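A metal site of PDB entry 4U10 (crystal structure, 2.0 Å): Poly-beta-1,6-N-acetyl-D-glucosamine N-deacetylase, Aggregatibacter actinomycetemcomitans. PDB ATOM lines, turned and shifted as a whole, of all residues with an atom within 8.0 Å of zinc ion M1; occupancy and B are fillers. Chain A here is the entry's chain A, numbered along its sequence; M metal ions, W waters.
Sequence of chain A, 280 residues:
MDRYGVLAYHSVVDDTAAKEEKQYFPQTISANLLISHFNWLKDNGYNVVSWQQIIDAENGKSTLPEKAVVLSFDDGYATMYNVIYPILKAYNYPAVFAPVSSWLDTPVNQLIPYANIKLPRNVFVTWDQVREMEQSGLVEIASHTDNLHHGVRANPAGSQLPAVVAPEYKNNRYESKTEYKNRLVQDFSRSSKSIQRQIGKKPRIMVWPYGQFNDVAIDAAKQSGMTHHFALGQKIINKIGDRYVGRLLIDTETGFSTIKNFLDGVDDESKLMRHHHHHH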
ATOM      1  N   TYR A   9       9.859  14.429 -29.096  1.00  0.00           N
ATOM      2  CA  TYR A   9      11.032  15.280 -29.123  1.00  0.00           C
ATOM      3  C   TYR A   9      12.214  14.525 -28.508  1.00  0.00           C
ATOM      4  O   TYR A   9      12.000  13.549 -27.845  1.00  0.00           O
ATOM      5  CB  TYR A   9      10.845  16.532 -28.257  1.00  0.00           C
ATOM      6  CG  TYR A   9       9.870  17.567 -28.838  1.00  0.00           C
ATOM      7  CD1 TYR A   9      10.296  18.573 -29.698  1.00  0.00           C
ATOM      8  CD2 TYR A   9       8.527  17.549 -28.460  1.00  0.00           C
ATOM      9  CE1 TYR A   9       9.370  19.479 -30.238  1.00  0.00           C
ATOM     10  CE2 TYR A   9       7.604  18.490 -28.958  1.00  0.00           C
ATOM     11  CZ  TYR A   9       8.002  19.413 -29.822  1.00  0.00           C
ATOM     12  OH  TYR A   9       7.036  20.314 -30.326  1.00  0.00           O
ATOM     13  N   HIS A  10      13.439  14.986 -28.765  1.00  0.00           N
ATOM     14  CA  HIS A  10      14.639  14.429 -28.122  1.00  0.00           C
ATOM     15  C   HIS A  10      15.345  15.576 -27.426  1.00  0.00           C
ATOM     16  O   HIS A  10      14.776  16.165 -26.460  1.00  0.00           O
ATOM     17  CB  HIS A  10      15.474  13.688 -29.185  1.00  0.00           C
ATOM     18  CG  HIS A  10      14.783  12.461 -29.675  1.00  0.00           C
ATOM     19  ND1 HIS A  10      13.765  12.523 -30.603  1.00  0.00           N
ATOM     20  CD2 HIS A  10      14.860  11.188 -29.284  1.00  0.00           C
ATOM     21  CE1 HIS A  10      13.270  11.323 -30.804  1.00  0.00           C
ATOM     22  NE2 HIS A  10      13.923  10.481 -30.022  1.00  0.00           N
ATOM     23  N   PHE A  73       9.414  13.462 -24.523  1.00  0.00           N
ATOM     24  CA  PHE A  73      10.826  13.760 -24.681  1.00  0.00           C
ATOM     25  C   PHE A  73      11.598  12.511 -24.348  1.00  0.00           C
ATOM     26  O   PHE A  73      11.348  11.868 -23.309  1.00  0.00           O
ATOM     27  CB  PHE A  73      11.283  14.915 -23.809  1.00  0.00           C
ATOM     28  CG  PHE A  73      10.576  16.202 -24.105  1.00  0.00           C
ATOM     29  CD1 PHE A  73       9.332  16.480 -23.514  1.00  0.00           C
ATOM     30  CD2 PHE A  73      11.147  17.153 -24.932  1.00  0.00           C
ATOM     31  CE1 PHE A  73       8.665  17.668 -23.841  1.00  0.00           C
ATOM     32  CE2 PHE A  73      10.489  18.318 -25.231  1.00  0.00           C
ATOM     33  CZ  PHE A  73       9.241  18.565 -24.703  1.00  0.00           C
ATOM     34  N   ASP A  74      12.401  12.072 -25.310  1.00  0.00           N
ATOM     35  CA  ASP A  74      13.139  10.813 -25.204  1.00  0.00           C
ATOM     36  C   ASP A  74      14.636  10.994 -24.904  1.00  0.00           C
ATOM     37  O   ASP A  74      15.283  11.869 -25.466  1.00  0.00           O
ATOM     38  CB  ASP A  74      13.112  10.008 -26.496  1.00  0.00           C
ATOM     39  CG  ASP A  74      11.734   9.493 -26.910  1.00  0.00           C
ATOM     40  OD1 ASP A  74      10.732   9.648 -26.182  1.00  0.00           O
ATOM     41  OD2 ASP A  74      11.714   8.847 -28.012  1.00  0.00           O
ATOM     42  N   ASP A  75      15.124  10.097 -24.012  1.00  0.00           N
ATOM     43  CA  ASP A  75      16.484   9.581 -23.896  1.00  0.00           C
ATOM     44  C   ASP A  75      17.167   9.875 -22.566  1.00  0.00           C
ATOM     45  O   ASP A  75      17.994   9.101 -22.161  1.00  0.00           O
ATOM     46  CB  ASP A  75      17.437  10.020 -25.010  1.00  0.00           C
ATOM     47  CG  ASP A  75      17.161   9.349 -26.283  1.00  0.00           C
ATOM     48  OD1 ASP A  75      16.143   8.674 -26.448  1.00  0.00           O
ATOM     49  OD2 ASP A  75      18.029   9.495 -27.159  1.00  0.00           O
ATOM     50  N   GLY A  76      16.759  10.927 -21.877  1.00  0.00           N
ATOM     51  CA  GLY A  76      17.421  11.324 -20.623  1.00  0.00           C
ATOM     52  C   GLY A  76      18.434  12.405 -20.763  1.00  0.00           C
ATOM     53  O   GLY A  76      19.214  12.597 -19.835  1.00  0.00           O
ATOM     54  N   TYR A  77      18.450  13.137 -21.884  1.00  0.00           N
ATOM     55  CA  TYR A  77      19.458  14.279 -22.001  1.00  0.00           C
ATOM     56  C   TYR A  77      19.285  15.324 -20.930  1.00  0.00           C
ATOM     57  O   TYR A  77      18.166  15.683 -20.634  1.00  0.00           O
ATOM     58  CB  TYR A  77      19.426  14.954 -23.366  1.00  0.00           C
ATOM     59  CG  TYR A  77      19.672  14.045 -24.549  1.00  0.00           C
ATOM     60  CD1 TYR A  77      20.893  13.376 -24.734  1.00  0.00           C
ATOM     61  CD2 TYR A  77      18.667  13.820 -25.477  1.00  0.00           C
ATOM     62  CE1 TYR A  77      21.076  12.539 -25.844  1.00  0.00           C
ATOM     63  CE2 TYR A  77      18.865  13.033 -26.531  1.00  0.00           C
ATOM     64  CZ  TYR A  77      20.058  12.383 -26.731  1.00  0.00           C
ATOM     65  OH  TYR A  77      20.163  11.582 -27.882  1.00  0.00           O
ATOM     66  N   ALA A  98      11.183  10.061 -21.115  1.00  0.00           N
ATOM     67  CA  ALA A  98      11.618   8.683 -21.158  1.00  0.00           C
ATOM     68  C   ALA A  98      13.150   8.526 -21.158  1.00  0.00           C
ATOM     69  O   ALA A  98      13.824   8.324 -22.205  1.00  0.00           O
ATOM     70  CB  ALA A  98      10.978   7.977 -22.320  1.00  0.00           C
ATOM     71  N   PRO A  99      13.723   8.610 -19.943  1.00  0.00           N
ATOM     72  CA  PRO A  99      15.161   8.404 -19.860  1.00  0.00           C
ATOM     73  C   PRO A  99      15.586   6.926 -19.921  1.00  0.00           C
ATOM     74  O   PRO A  99      14.927   6.046 -19.378  1.00  0.00           O
ATOM     75  CB  PRO A  99      15.486   9.058 -18.498  1.00  0.00           C
ATOM     76  CG  PRO A  99      14.269   8.614 -17.656  1.00  0.00           C
ATOM     77  CD  PRO A  99      13.112   8.814 -18.625  1.00  0.00           C
ATOM     78  N   VAL A 100      16.706   6.624 -20.584  1.00  0.00           N
ATOM     79  CA  VAL A 100      17.250   5.323 -20.498  1.00  0.00           C
ATOM     80  C   VAL A 100      17.775   5.097 -19.083  1.00  0.00           C
ATOM     81  O   VAL A 100      18.686   5.777 -18.651  1.00  0.00           O
ATOM     82  CB  VAL A 100      18.358   5.147 -21.508  1.00  0.00           C
ATOM     83  CG1 VAL A 100      18.941   3.728 -21.385  1.00  0.00           C
ATOM     84  CG2 VAL A 100      17.854   5.392 -22.952  1.00  0.00           C
ATOM     85  N   TRP A 103      21.631   4.544 -18.138  1.00  0.00           N
ATOM     86  CA  TRP A 103      22.405   5.768 -18.326  1.00  0.00           C
ATOM     87  C   TRP A 103      22.314   6.596 -17.027  1.00  0.00           C
ATOM     88  O   TRP A 103      23.338   6.967 -16.444  1.00  0.00           O
ATOM     89  CB  TRP A 103      21.932   6.550 -19.582  1.00  0.00           C
ATOM     90  CG  TRP A 103      22.156   5.856 -20.825  1.00  0.00           C
ATOM     91  CD1 TRP A 103      22.899   4.672 -20.998  1.00  0.00           C
ATOM     92  CD2 TRP A 103      21.696   6.234 -22.115  1.00  0.00           C
ATOM     93  NE1 TRP A 103      22.884   4.332 -22.319  1.00  0.00           N
ATOM     94  CE2 TRP A 103      22.149   5.262 -23.022  1.00  0.00           C
ATOM     95  CE3 TRP A 103      20.895   7.294 -22.605  1.00  0.00           C
ATOM     96  CZ2 TRP A 103      21.881   5.336 -24.376  1.00  0.00           C
ATOM     97  CZ3 TRP A 103      20.616   7.360 -23.956  1.00  0.00           C
ATOM     98  CH2 TRP A 103      21.122   6.409 -24.819  1.00  0.00           C
ATOM     99  N   TYR A 114      28.621   3.960 -25.575  1.00  0.00           N
ATOM    100  CA  TYR A 114      27.570   4.318 -26.517  1.00  0.00           C
ATOM    101  C   TYR A 114      28.089   4.116 -27.948  1.00  0.00           C
ATOM    102  O   TYR A 114      28.835   4.957 -28.461  1.00  0.00           O
ATOM    103  CB  TYR A 114      27.154   5.761 -26.275  1.00  0.00           C
ATOM    104  CG  TYR A 114      25.883   6.216 -26.956  1.00  0.00           C
ATOM    105  CD1 TYR A 114      25.792   6.357 -28.350  1.00  0.00           C
ATOM    106  CD2 TYR A 114      24.792   6.602 -26.196  1.00  0.00           C
ATOM    107  CE1 TYR A 114      24.631   6.802 -28.968  1.00  0.00           C
ATOM    108  CE2 TYR A 114      23.634   7.072 -26.801  1.00  0.00           C
ATOM    109  CZ  TYR A 114      23.548   7.168 -28.170  1.00  0.00           C
ATOM    110  OH  TYR A 114      22.381   7.633 -28.700  1.00  0.00           O
ATOM    111  N   HIS A 144      12.372   3.808 -21.247  1.00  0.00           N
ATOM    112  CA  HIS A 144      12.949   3.792 -22.584  1.00  0.00           C
ATOM    113  C   HIS A 144      14.012   2.690 -22.587  1.00  0.00           C
ATOM    114  O   HIS A 144      15.028   2.782 -23.303  1.00  0.00           O
ATOM    115  CB  HIS A 144      13.593   5.135 -22.860  1.00  0.00           C
ATOM    116  CG  HIS A 144      13.792   5.500 -24.298  1.00  0.00           C
ATOM    117  ND1 HIS A 144      12.883   5.228 -25.310  1.00  0.00           N
ATOM    118  CD2 HIS A 144      14.715   6.308 -24.860  1.00  0.00           C
ATOM    119  CE1 HIS A 144      13.284   5.782 -26.419  1.00  0.00           C
ATOM    120  NE2 HIS A 144      14.385   6.465 -26.176  1.00  0.00           N
ATOM    121  N   THR A 145      13.686   1.589 -21.888  1.00  0.00           N
ATOM    122  CA  THR A 145      14.501   0.384 -21.635  1.00  0.00           C
ATOM    123  C   THR A 145      15.548   0.725 -20.600  1.00  0.00           C
ATOM    124  O   THR A 145      15.697   1.872 -20.272  1.00  0.00           O
ATOM    125  CB  THR A 145      15.161  -0.269 -22.889  1.00  0.00           C
ATOM    126  OG1 THR A 145      16.256   0.537 -23.288  1.00  0.00           O
ATOM    127  CG2 THR A 145      14.142  -0.305 -24.049  1.00  0.00           C
ATOM    128  N   HIS A 149      18.978   0.574 -25.629  1.00  0.00           N
ATOM    129  CA  HIS A 149      18.964   1.715 -26.516  1.00  0.00           C
ATOM    130  C   HIS A 149      20.269   1.684 -27.267  1.00  0.00           C
ATOM    131  O   HIS A 149      21.060   2.634 -27.195  1.00  0.00           O
ATOM    132  CB  HIS A 149      18.898   2.978 -25.712  1.00  0.00           C
ATOM    133  CG  HIS A 149      18.395   4.140 -26.481  1.00  0.00           C
ATOM    134  ND1 HIS A 149      19.094   4.755 -27.486  1.00  0.00           N
ATOM    135  CD2 HIS A 149      17.211   4.803 -26.401  1.00  0.00           C
ATOM    136  CE1 HIS A 149      18.385   5.724 -28.002  1.00  0.00           C
ATOM    137  NE2 HIS A 149      17.255   5.812 -27.320  1.00  0.00           N
ATOM    138  N   VAL A 207       8.476   3.582 -23.945  1.00  0.00           N
ATOM    139  CA  VAL A 207       8.758   4.260 -25.185  1.00  0.00           C
ATOM    140  C   VAL A 207       9.849   3.550 -25.932  1.00  0.00           C
ATOM    141  O   VAL A 207      10.975   3.391 -25.419  1.00  0.00           O
ATOM    142  CB  VAL A 207       9.138   5.738 -24.946  1.00  0.00           C
ATOM    143  CG1 VAL A 207       9.320   6.444 -26.287  1.00  0.00           C
ATOM    144  CG2 VAL A 207       8.090   6.472 -24.083  1.00  0.00           C
ATOM    145  N   TRP A 208       9.592   3.189 -27.194  1.00  0.00           N
ATOM    146  CA  TRP A 208      10.548   2.308 -27.920  1.00  0.00           C
ATOM    147  C   TRP A 208      11.683   3.135 -28.433  1.00  0.00           C
ATOM    148  O   TRP A 208      11.435   4.207 -29.056  1.00  0.00           O
ATOM    149  CB  TRP A 208       9.843   1.661 -29.109  1.00  0.00           C
ATOM    150  CG  TRP A 208       8.637   0.853 -28.716  1.00  0.00           C
ATOM    151  CD1 TRP A 208       7.356   1.052 -29.152  1.00  0.00           C
ATOM    152  CD2 TRP A 208       8.600  -0.294 -27.856  1.00  0.00           C
ATOM    153  NE1 TRP A 208       6.541   0.110 -28.581  1.00  0.00           N
ATOM    154  CE2 TRP A 208       7.277  -0.711 -27.778  1.00  0.00           C
ATOM    155  CE3 TRP A 208       9.569  -0.985 -27.105  1.00  0.00           C
ATOM    156  CZ2 TRP A 208       6.885  -1.778 -26.993  1.00  0.00           C
ATOM    157  CZ3 TRP A 208       9.179  -2.020 -26.353  1.00  0.00           C
ATOM    158  CH2 TRP A 208       7.847  -2.423 -26.300  1.00  0.00           C
ATOM    159  N   PRO A 209      12.942   2.705 -28.183  1.00  0.00           N
ATOM    160  CA  PRO A 209      14.076   3.322 -28.879  1.00  0.00           C
ATOM    161  C   PRO A 209      13.880   3.319 -30.379  1.00  0.00           C
ATOM    162  O   PRO A 209      13.535   2.263 -30.961  1.00  0.00           O
ATOM    163  CB  PRO A 209      15.246   2.358 -28.509  1.00  0.00           C
ATOM    164  CG  PRO A 209      14.917   2.008 -27.092  1.00  0.00           C
ATOM    165  CD  PRO A 209      13.437   1.659 -27.262  1.00  0.00           C
ATOM    166  N   TYR A 210      14.091   4.476 -31.007  1.00  0.00           N
ATOM    167  CA  TYR A 210      14.042   4.648 -32.455  1.00  0.00           C
ATOM    168  C   TYR A 210      12.671   4.331 -33.000  1.00  0.00           C
ATOM    169  O   TYR A 210      12.519   4.116 -34.177  1.00  0.00           O
ATOM    170  CB  TYR A 210      15.093   3.704 -33.122  1.00  0.00           C
ATOM    171  CG  TYR A 210      16.465   3.586 -32.389  1.00  0.00           C
ATOM    172  CD1 TYR A 210      17.317   4.638 -32.280  1.00  0.00           C
ATOM    173  CD2 TYR A 210      16.880   2.367 -31.841  1.00  0.00           C
ATOM    174  CE1 TYR A 210      18.537   4.511 -31.613  1.00  0.00           C
ATOM    175  CE2 TYR A 210      18.109   2.227 -31.211  1.00  0.00           C
ATOM    176  CZ  TYR A 210      18.943   3.303 -31.099  1.00  0.00           C
ATOM    177  OH  TYR A 210      20.171   3.154 -30.466  1.00  0.00           O
ATOM    178  N   GLY A 211      11.638   4.248 -32.170  1.00  0.00           N
ATOM    179  CA  GLY A 211      10.300   3.967 -32.728  1.00  0.00           C
ATOM    180  C   GLY A 211      10.059   2.480 -33.022  1.00  0.00           C
ATOM    181  O   GLY A 211       8.998   2.132 -33.485  1.00  0.00           O
ATOM    182  N   ARG A 247       3.209   8.615 -32.566  1.00  0.00           N
ATOM    183  CA  ARG A 247       3.763   9.901 -32.312  1.00  0.00           C
ATOM    184  C   ARG A 247       4.317  10.500 -33.590  1.00  0.00           C
ATOM    185  O   ARG A 247       4.784   9.787 -34.511  1.00  0.00           O
ATOM    186  CB  ARG A 247       4.869   9.796 -31.235  1.00  0.00           C
ATOM    187  CG  ARG A 247       4.469   9.129 -29.898  1.00  0.00           C
ATOM    188  CD  ARG A 247       5.586   9.356 -28.870  1.00  0.00           C
ATOM    189  NE  ARG A 247       6.832   8.652 -29.277  1.00  0.00           N
ATOM    190  CZ  ARG A 247       8.028   8.817 -28.727  1.00  0.00           C
ATOM    191  NH1 ARG A 247       8.209   9.686 -27.737  1.00  0.00           N
ATOM    192  NH2 ARG A 247       9.086   8.146 -29.179  1.00  0.00           N
HETATM  193 ZN    ZN M   1      15.754   7.201 -27.586  1.00  0.00          ZN
HETATM  194 ZN    ZN M   2      13.187   8.534 -29.457  1.00  0.00          ZN
HETATM  195  O   HOH W   1      14.645   7.213 -29.096  1.00  0.00           O
HETATM  196  O   HOH W   2      17.407   8.440 -29.409  1.00  0.00           O
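Water W1 is bound to zinc ion M1 (1.9 Å). OD1 of Asp 75 is bound to zinc ion M1 (1.9 Å). NE2 of His 149 binds zinc ion M1, 2.1 Å away. Zinc ion M1 is bound by NE2 of His 144, 2.1 Å away. Zinc ion M1 has four donor atoms within binding distance. Slightly farther from zinc ion M1 lies water W2 (2.8 Å).
Within 4 Å of zinc ion M1: Asp 75, His 144 and His 149.
The backbone NH (N) of Val 100 lies within hydrogen-bond range of the backbone carbonyl oxygen (O) of Asp 75 (3.2 Å). The backbone carbonyl oxygen of Ala 98 lies within hydrogen-bond range of the backbone NH of Asp 75. OD2 of Asp 75 is in hydrogen-bond range of OH of Tyr 77 (3.1 Å). The side-chain hydroxyl (OH) of Tyr 210 sits at hydrogen-bond distance from the backbone carbonyl oxygen (O) of His 149, 3.4 Å away. The backbone carbonyl oxygen (O) of Val 207 is in hydrogen-bond range of a ring nitrogen (ND1) of His 144, 2.7 Å away.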
